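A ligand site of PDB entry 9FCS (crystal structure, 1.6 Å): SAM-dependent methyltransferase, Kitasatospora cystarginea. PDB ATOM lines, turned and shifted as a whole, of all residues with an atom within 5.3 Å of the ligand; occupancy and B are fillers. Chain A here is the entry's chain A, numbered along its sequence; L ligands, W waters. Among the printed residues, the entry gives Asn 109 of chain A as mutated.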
ATOM      1  N   TYR A   4      -6.940  13.424  -7.644  1.00  0.00           N
ATOM      2  CA  TYR A   4      -5.650  13.216  -6.934  1.00  0.00           C
ATOM      3  C   TYR A   4      -4.658  12.508  -7.869  1.00  0.00           C
ATOM      4  O   TYR A   4      -3.503  12.964  -7.959  1.00  0.00           O
ATOM      5  CB  TYR A   4      -5.835  12.428  -5.633  1.00  0.00           C
ATOM      6  CG  TYR A   4      -4.523  12.091  -4.956  1.00  0.00           C
ATOM      7  CD1 TYR A   4      -3.960  12.952  -4.019  1.00  0.00           C
ATOM      8  CD2 TYR A   4      -3.827  10.940  -5.277  1.00  0.00           C
ATOM      9  CE1 TYR A   4      -2.747  12.667  -3.410  1.00  0.00           C
ATOM     10  CE2 TYR A   4      -2.612  10.640  -4.677  1.00  0.00           C
ATOM     11  CZ  TYR A   4      -2.074  11.499  -3.742  1.00  0.00           C
ATOM     12  OH  TYR A   4      -0.884  11.205  -3.155  1.00  0.00           O
ATOM     13  N   ARG A   8      -1.061  13.925  -9.420  1.00  0.00           N
ATOM     14  CA  ARG A   8       0.251  13.246  -9.283  1.00  0.00           C
ATOM     15  C   ARG A   8       0.933  13.207 -10.654  1.00  0.00           C
ATOM     16  O   ARG A   8       2.158  13.455 -10.719  1.00  0.00           O
ATOM     17  CB  ARG A   8       0.086  11.864  -8.644  1.00  0.00           C
ATOM     18  CG  ARG A   8      -0.493  11.884  -7.244  1.00  0.00           C
ATOM     19  CD  ARG A   8       0.227  12.795  -6.275  1.00  0.00           C
ATOM     20  NE  ARG A   8       1.587  12.349  -5.996  1.00  0.00           N
ATOM     21  CZ  ARG A   8       2.512  13.045  -5.351  1.00  0.00           C
ATOM     22  NH1 ARG A   8       2.250  14.259  -4.896  1.00  0.00           N
ATOM     23  NH2 ARG A   8       3.711  12.526  -5.153  1.00  0.00           N
ATOM     24  N   TYR A  19       6.607   4.666 -12.824  1.00  0.00           N
ATOM     25  CA  TYR A  19       5.734   3.713 -12.087  1.00  0.00           C
ATOM     26  C   TYR A  19       5.611   2.420 -12.906  1.00  0.00           C
ATOM     27  O   TYR A  19       5.686   1.319 -12.320  1.00  0.00           O
ATOM     28  CB  TYR A  19       4.385   4.330 -11.750  1.00  0.00           C
ATOM     29  CG  TYR A  19       4.381   5.220 -10.536  1.00  0.00           C
ATOM     30  CD1 TYR A  19       3.781   4.812  -9.344  1.00  0.00           C
ATOM     31  CD2 TYR A  19       4.984   6.459 -10.551  1.00  0.00           C
ATOM     32  CE1 TYR A  19       3.761   5.626  -8.221  1.00  0.00           C
ATOM     33  CE2 TYR A  19       4.988   7.283  -9.438  1.00  0.00           C
ATOM     34  CZ  TYR A  19       4.367   6.866  -8.269  1.00  0.00           C
ATOM     35  OH  TYR A  19       4.361   7.679  -7.172  1.00  0.00           O
ATOM     36  N   ASP A  38       4.423  -2.530   0.116  1.00  0.00           N
ATOM     37  CA  ASP A  38       4.535  -1.139  -0.408  1.00  0.00           C
ATOM     38  C   ASP A  38       4.834  -0.218   0.777  1.00  0.00           C
ATOM     39  O   ASP A  38       3.913  -0.015   1.588  1.00  0.00           O
ATOM     40  CB  ASP A  38       3.261  -0.764  -1.170  1.00  0.00           C
ATOM     41  CG  ASP A  38       3.319   0.583  -1.883  1.00  0.00           C
ATOM     42  OD1 ASP A  38       4.407   1.202  -1.876  1.00  0.00           O
ATOM     43  OD2 ASP A  38       2.272   0.997  -2.443  1.00  0.00           O
ATOM     44  N   LEU A  39       6.089   0.248   0.895  1.00  0.00           N
ATOM     45  CA  LEU A  39       6.582   1.119   2.006  1.00  0.00           C
ATOM     46  C   LEU A  39       6.275   2.583   1.688  1.00  0.00           C
ATOM     47  O   LEU A  39       6.716   3.056   0.631  1.00  0.00           O
ATOM     48  CB  LEU A  39       8.091   0.941   2.180  1.00  0.00           C
ATOM     49  CG  LEU A  39       8.559  -0.184   3.088  1.00  0.00           C
ATOM     50  CD1 LEU A  39      10.077  -0.237   3.133  1.00  0.00           C
ATOM     51  CD2 LEU A  39       7.994  -0.013   4.494  1.00  0.00           C
ATOM     52  N   GLY A  40       5.589   3.287   2.587  1.00  0.00           N
ATOM     53  CA  GLY A  40       5.133   4.674   2.346  1.00  0.00           C
ATOM     54  C   GLY A  40       4.104   4.700   1.224  1.00  0.00           C
ATOM     55  O   GLY A  40       4.218   5.565   0.336  1.00  0.00           O
ATOM     56  N   ALA A  41       3.153   3.769   1.278  1.00  0.00           N
ATOM     57  CA  ALA A  41       2.158   3.472   0.233  1.00  0.00           C
ATOM     58  C   ALA A  41       1.273   4.685  -0.063  1.00  0.00           C
ATOM     59  O   ALA A  41       0.693   4.726  -1.157  1.00  0.00           O
ATOM     60  CB  ALA A  41       1.311   2.293   0.640  1.00  0.00           C
ATOM     61  N   GLY A  42       1.121   5.622   0.887  1.00  0.00           N
ATOM     62  CA  GLY A  42       0.229   6.778   0.731  1.00  0.00           C
ATOM     63  C   GLY A  42      -1.174   6.336   0.384  1.00  0.00           C
ATOM     64  O   GLY A  42      -1.736   5.494   1.110  1.00  0.00           O
ATOM     65  N   THR A  43      -1.731   6.867  -0.705  1.00  0.00           N
ATOM     66  CA  THR A  43      -3.097   6.524  -1.199  1.00  0.00           C
ATOM     67  C   THR A  43      -3.072   5.185  -1.947  1.00  0.00           C
ATOM     68  O   THR A  43      -4.147   4.777  -2.397  1.00  0.00           O
ATOM     69  CB  THR A  43      -3.680   7.633  -2.084  1.00  0.00           C
ATOM     70  OG1 THR A  43      -2.984   7.621  -3.335  1.00  0.00           O
ATOM     71  CG2 THR A  43      -3.602   9.007  -1.465  1.00  0.00           C
ATOM     72  N   GLY A  44      -1.898   4.572  -2.113  1.00  0.00           N
ATOM     73  CA  GLY A  44      -1.756   3.203  -2.651  1.00  0.00           C
ATOM     74  C   GLY A  44      -1.585   3.184  -4.162  1.00  0.00           C
ATOM     75  O   GLY A  44      -1.893   2.143  -4.767  1.00  0.00           O
ATOM     76  N   LEU A  45      -1.070   4.266  -4.766  1.00  0.00           N
ATOM     77  CA  LEU A  45      -0.907   4.397  -6.230  1.00  0.00           C
ATOM     78  C   LEU A  45       0.007   3.297  -6.779  1.00  0.00           C
ATOM     79  O   LEU A  45      -0.372   2.678  -7.785  1.00  0.00           O
ATOM     80  CB  LEU A  45      -0.353   5.777  -6.592  1.00  0.00           C
ATOM     81  CG  LEU A  45      -1.403   6.846  -6.914  1.00  0.00           C
ATOM     82  CD1 LEU A  45      -0.740   8.179  -7.180  1.00  0.00           C
ATOM     83  CD2 LEU A  45      -2.258   6.423  -8.098  1.00  0.00           C
ATOM     84  N   LEU A  46       1.171   3.053  -6.168  1.00  0.00           N
ATOM     85  CA  LEU A  46       2.105   2.015  -6.668  1.00  0.00           C
ATOM     86  C   LEU A  46       1.479   0.628  -6.462  1.00  0.00           C
ATOM     87  O   LEU A  46       1.508  -0.183  -7.407  1.00  0.00           O
ATOM     88  CB  LEU A  46       3.469   2.127  -5.978  1.00  0.00           C
ATOM     89  CG  LEU A  46       4.527   1.139  -6.488  1.00  0.00           C
ATOM     90  CD1 LEU A  46       4.650   1.192  -8.002  1.00  0.00           C
ATOM     91  CD2 LEU A  46       5.875   1.390  -5.834  1.00  0.00           C
ATOM     92  N   ASP A  63       2.335   2.723   5.844  1.00  0.00           N
ATOM     93  CA  ASP A  63       2.565   4.184   5.879  1.00  0.00           C
ATOM     94  C   ASP A  63       2.412   4.623   7.332  1.00  0.00           C
ATOM     95  O   ASP A  63       1.749   3.907   8.098  1.00  0.00           O
ATOM     96  CB  ASP A  63       1.589   4.911   4.958  1.00  0.00           C
ATOM     97  CG  ASP A  63       2.052   6.277   4.502  1.00  0.00           C
ATOM     98  OD1 ASP A  63       2.444   6.393   3.333  1.00  0.00           O
ATOM     99  OD2 ASP A  63       2.011   7.213   5.326  1.00  0.00           O
ATOM    100  N   ARG A  64       2.997   5.754   7.694  1.00  0.00           N
ATOM    101  CA  ARG A  64       2.819   6.290   9.067  1.00  0.00           C
ATOM    102  C   ARG A  64       1.521   7.112   9.140  1.00  0.00           C
ATOM    103  O   ARG A  64       1.064   7.328  10.263  1.00  0.00           O
ATOM    104  CB  ARG A  64       4.016   7.129   9.485  1.00  0.00           C
ATOM    105  CG  ARG A  64       4.171   8.438   8.731  1.00  0.00           C
ATOM    106  CD  ARG A  64       5.329   9.146   9.376  1.00  0.00           C
ATOM    107  NE  ARG A  64       5.729  10.365   8.708  1.00  0.00           N
ATOM    108  CZ  ARG A  64       6.848  11.019   8.999  1.00  0.00           C
ATOM    109  NH1 ARG A  64       7.670  10.566   9.937  1.00  0.00           N
ATOM    110  NH2 ARG A  64       7.140  12.125   8.333  1.00  0.00           N
ATOM    111  N   SER A  65       0.961   7.542   8.003  1.00  0.00           N
ATOM    112  CA  SER A  65      -0.214   8.445   7.944  1.00  0.00           C
ATOM    113  C   SER A  65      -1.512   7.641   7.783  1.00  0.00           C
ATOM    114  O   SER A  65      -1.742   7.099   6.700  1.00  0.00           O
ATOM    115  CB  SER A  65      -0.091   9.475   6.867  1.00  0.00           C
ATOM    116  OG  SER A  65      -1.315  10.175   6.727  1.00  0.00           O
ATOM    117  N   MET A  68      -3.578   9.248   4.852  1.00  0.00           N
ATOM    118  CA  MET A  68      -3.196   8.742   3.508  1.00  0.00           C
ATOM    119  C   MET A  68      -3.754   7.331   3.327  1.00  0.00           C
ATOM    120  O   MET A  68      -4.347   7.053   2.263  1.00  0.00           O
ATOM    121  CB  MET A  68      -1.667   8.740   3.316  1.00  0.00           C
ATOM    122  CG  MET A  68      -1.064  10.124   3.344  1.00  0.00           C
ATOM    123  SD  MET A  68      -1.583  11.153   1.954  1.00  0.00           S
ATOM    124  CE  MET A  68      -0.647  10.399   0.627  1.00  0.00           C
ATOM    125  N   ALA A  87       2.809   2.182  10.285  1.00  0.00           N
ATOM    126  CA  ALA A  87       4.175   2.135  10.847  1.00  0.00           C
ATOM    127  C   ALA A  87       5.073   3.152  10.134  1.00  0.00           C
ATOM    128  O   ALA A  87       4.932   3.333   8.913  1.00  0.00           O
ATOM    129  CB  ALA A  87       4.737   0.738  10.729  1.00  0.00           C
ATOM    130  N   ASP A  88       5.988   3.752  10.894  1.00  0.00           N
ATOM    131  CA  ASP A  88       7.070   4.608  10.363  1.00  0.00           C
ATOM    132  C   ASP A  88       8.103   3.686   9.703  1.00  0.00           C
ATOM    133  O   ASP A  88       8.233   2.532  10.136  1.00  0.00           O
ATOM    134  CB  ASP A  88       7.706   5.438  11.482  1.00  0.00           C
ATOM    135  CG  ASP A  88       8.458   6.655  10.964  1.00  0.00           C
ATOM    136  OD1 ASP A  88       7.906   7.765  11.100  1.00  0.00           O
ATOM    137  OD2 ASP A  88       9.584   6.481  10.451  1.00  0.00           O
ATOM    138  N   HIS A  89       8.815   4.178   8.684  1.00  0.00           N
ATOM    139  CA  HIS A  89       9.963   3.464   8.090  1.00  0.00           C
ATOM    140  C   HIS A  89      10.959   3.066   9.182  1.00  0.00           C
ATOM    141  O   HIS A  89      11.638   2.045   8.988  1.00  0.00           O
ATOM    142  CB  HIS A  89      10.686   4.304   7.026  1.00  0.00           C
ATOM    143  CG  HIS A  89       9.830   4.735   5.889  1.00  0.00           C
ATOM    144  ND1 HIS A  89       8.710   4.035   5.476  1.00  0.00           N
ATOM    145  CD2 HIS A  89       9.938   5.797   5.060  1.00  0.00           C
ATOM    146  CE1 HIS A  89       8.166   4.655   4.445  1.00  0.00           C
ATOM    147  NE2 HIS A  89       8.898   5.741   4.180  1.00  0.00           N
ATOM    148  N   LEU A  90      11.072   3.858  10.250  1.00  0.00           N
ATOM    149  CA  LEU A  90      12.081   3.665  11.339  1.00  0.00           C
ATOM    150  C   LEU A  90      11.585   2.627  12.360  1.00  0.00           C
ATOM    151  O   LEU A  90      12.423   2.173  13.163  1.00  0.00           O
ATOM    152  CB  LEU A  90      12.359   5.014  12.018  1.00  0.00           C
ATOM    153  CG  LEU A  90      12.900   6.122  11.110  1.00  0.00           C
ATOM    154  CD1 LEU A  90      13.213   7.363  11.921  1.00  0.00           C
ATOM    155  CD2 LEU A  90      14.138   5.659  10.351  1.00  0.00           C
ATOM    156  N   ALA A 104       7.512   4.344  -3.426  1.00  0.00           N
ATOM    157  CA  ALA A 104       7.466   5.473  -4.381  1.00  0.00           C
ATOM    158  C   ALA A 104       7.413   6.778  -3.597  1.00  0.00           C
ATOM    159  O   ALA A 104       6.490   6.942  -2.769  1.00  0.00           O
ATOM    160  CB  ALA A 104       6.294   5.325  -5.329  1.00  0.00           C
ATOM    161  N   LEU A 105       8.418   7.632  -3.809  1.00  0.00           N
ATOM    162  CA  LEU A 105       8.466   9.056  -3.369  1.00  0.00           C
ATOM    163  C   LEU A 105       8.249   9.170  -1.856  1.00  0.00           C
ATOM    164  O   LEU A 105       7.497  10.054  -1.422  1.00  0.00           O
ATOM    165  CB  LEU A 105       7.419   9.844  -4.167  1.00  0.00           C
ATOM    166  CG  LEU A 105       7.555   9.758  -5.687  1.00  0.00           C
ATOM    167  CD1 LEU A 105       6.455  10.555  -6.370  1.00  0.00           C
ATOM    168  CD2 LEU A 105       8.923  10.241  -6.138  1.00  0.00           C
ATOM    169  N   SER A 106       8.933   8.325  -1.079  1.00  0.00           N
ATOM    170  CA  SER A 106       8.752   8.248   0.395  1.00  0.00           C
ATOM    171  C   SER A 106      10.099   8.246   1.129  1.00  0.00           C
ATOM    172  O   SER A 106      10.205   8.913   2.174  1.00  0.00           O
ATOM    173  CB  SER A 106       7.932   7.042   0.742  1.00  0.00           C
ATOM    174  OG  SER A 106       7.529   7.096   2.106  1.00  0.00           O
ATOM    175  N   ASN A 109      12.448  11.203   2.471  1.00  0.00           N
ATOM    176  CA  ASN A 109      12.046  11.938   3.702  1.00  0.00           C
ATOM    177  C   ASN A 109      12.966  11.585   4.891  1.00  0.00           C
ATOM    178  O   ASN A 109      12.927  12.338   5.891  1.00  0.00           O
ATOM    179  CB  ASN A 109      10.575  11.672   4.041  1.00  0.00           C
ATOM    180  CG  ASN A 109       9.638  12.239   3.000  1.00  0.00           C
ATOM    181  OD1 ASN A 109       8.925  11.499   2.326  1.00  0.00           O
ATOM    182  ND2 ASN A 109       9.638  13.561   2.860  1.00  0.00           N
ATOM    183  N   LEU A 110      13.752  10.508   4.794  1.00  0.00           N
ATOM    184  CA  LEU A 110      14.630  10.001   5.892  1.00  0.00           C
ATOM    185  C   LEU A 110      16.003  10.653   5.811  1.00  0.00           C
ATOM    186  O   LEU A 110      16.452  10.961   4.689  1.00  0.00           O
ATOM    187  CB  LEU A 110      14.772   8.486   5.772  1.00  0.00           C
ATOM    188  CG  LEU A 110      13.497   7.660   5.917  1.00  0.00           C
ATOM    189  CD1 LEU A 110      13.822   6.181   5.780  1.00  0.00           C
ATOM    190  CD2 LEU A 110      12.796   7.936   7.239  1.00  0.00           C
HETATM  191  N1  LIG L   1       3.866   5.993  -2.403  1.00  0.00           N
HETATM  192  C1  LIG L   1       2.689   6.888  -2.610  1.00  0.00           C
HETATM  193  C2  LIG L   1       2.730   8.109  -1.687  1.00  0.00           C
HETATM  194  C3  LIG L   1       3.935   9.013  -1.883  1.00  0.00           C
HETATM  195  S1  LIG L   1       3.853  10.467  -0.809  1.00  0.00           S
HETATM  196  C4  LIG L   1       2.648   7.347  -4.081  1.00  0.00           C
HETATM  197  O1  LIG L   1       3.463   6.918  -4.895  1.00  0.00           O
HETATM  198  O2  LIG L   1       1.770   8.151  -4.448  1.00  0.00           O
HETATM  199  C5  LIG L   1       4.926  10.024   0.573  1.00  0.00           C
HETATM  200  C6  LIG L   1       4.291   9.075   1.567  1.00  0.00           C
HETATM  201  O3  LIG L   1       5.313   8.642   2.494  1.00  0.00           O
HETATM  202  C7  LIG L   1       3.173   9.686   2.422  1.00  0.00           C
HETATM  203  O4  LIG L   1       2.042   8.812   2.436  1.00  0.00           O
HETATM  204  C8  LIG L   1       3.818   9.855   3.796  1.00  0.00           C
HETATM  205  O5  LIG L   1       2.917   9.752   4.880  1.00  0.00           O
HETATM  206  C9  LIG L   1       4.802   8.698   3.800  1.00  0.00           C
HETATM  207  N2  LIG L   1       5.923   8.833   4.714  1.00  0.00           N
HETATM  208  C10 LIG L   1       6.832   9.869   4.779  1.00  0.00           C
HETATM  209  N3  LIG L   1       7.758   9.687   5.682  1.00  0.00           N
HETATM  210  C11 LIG L   1       7.451   8.461   6.253  1.00  0.00           C
HETATM  211  C12 LIG L   1       8.066   7.709   7.267  1.00  0.00           C
HETATM  212  N4  LIG L   1       9.159   8.100   7.918  1.00  0.00           N
HETATM  213  N5  LIG L   1       7.509   6.519   7.592  1.00  0.00           N
HETATM  214  C13 LIG L   1       6.412   6.126   6.932  1.00  0.00           C
HETATM  215  N6  LIG L   1       5.758   6.747   5.951  1.00  0.00           N
HETATM  216  C14 LIG L   1       6.336   7.916   5.654  1.00  0.00           C
HETATM  217  O   HOH W   1       2.675   9.792  -6.341  1.00  0.00           O
HETATM  218  O   HOH W   2       2.042   3.608  -3.290  1.00  0.00           O
HETATM  219  O   HOH W   3      -0.454   8.401  -2.986  1.00  0.00           O
HETATM  220  O   HOH W   4       5.201   3.649  -1.708  1.00  0.00           O
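N of Gly 42 sits at hydrogen-bond distance from OD1 of Asp 63 (2.9 Å). OD1 of Asp 63 sits at hydrogen-bond distance from N of Ala 41 (3.4 Å). A ring nitrogen (NE2) of His 89 lies within hydrogen-bond range of the side-chain hydroxyl (OG) of Ser 106. O of Ser 106 sits close to OD1 of Asn 109. The guanidinium group of Arg 64 lies within salt-bridge range of the side-chain carboxylate of Asp 88 (3.0 Å). N of Leu 90 lies within hydrogen-bond range of OD2 of Asp 88, at 3.0 Å. N of Arg 64 lies within hydrogen-bond range of O of Ala 87. The backbone NH (N) of Met 68 lies within hydrogen-bond range of the side-chain hydroxyl (OG) of Ser 65 (3.1 Å).
OH of Tyr 19 is in hydrogen-bond range of O1 of the ligand (2.6 Å). The side-chain carboxylate (OD1) of Asp 63 is in hydrogen-bond range of an oxygen (O4) of the ligand (2.6 Å). An oxygen (O3) of the ligand lies within hydrogen-bond range of the side-chain hydroxyl (OG) of Ser 106 (2.7 Å). O of Gly 40 lies within hydrogen-bond range of N1 of the ligand, 2.8 Å away. The backbone carbonyl oxygen of Ala 104 is in hydrogen-bond range of a nitrogen (N1) of the ligand. The backbone NH (N) of His 89 lies within hydrogen-bond range of a nitrogen (N5) of the ligand (2.9 Å). A nitrogen (N5) of the ligand lies close to a ring nitrogen (ND1) of His 89, 3.5 Å away. A nitrogen (N4) of the ligand sits at hydrogen-bond distance from the side-chain carboxylate of Asp 88, 3.0 Å away. A nitrogen (N6) of the ligand is in hydrogen-bond range of the backbone NH (N) of Arg 64.
The backbone carbonyl oxygen (O) of Leu 105 lies close to a sulfur (S1) of the ligand (3.7 Å). Ala 41 touches the ligand. Gly 42 touches the ligand. Leu 45 touches the ligand. CB of Ser 65 touches O5 of the ligand (3.6 Å). Met 68 touches the ligand (CG to O4, 3.5 Å). O of Ala 87 touches C13 of the ligand (3.7 Å). Asn 109 touches the ligand (OD1 to C10, 3.6 Å). Leu 110 touches the ligand (CD2 to N4, 3.7 Å). Along chain A the residues within 4 Å of the ligand span positions 19 to 110.
Water W1 lies within hydrogen-bond range of an oxygen (O2) of the ligand (2.7 Å), the guanidinium group of Arg 8 (2.8 Å) and the side-chain hydroxyl of Tyr 19 (2.8 Å). Water W3 lies within hydrogen-bond range of OG1 of Thr 43, O2 of the ligand and OH of Tyr 4. Water W2 lies within hydrogen-bond range of the side-chain carboxylate of Asp 38 (2.8 Å), the backbone carbonyl oxygen of Ala 41 (2.8 Å), the backbone NH of Leu 46 (3.1 Å) and a nitrogen (N1) of the ligand (3.1 Å).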
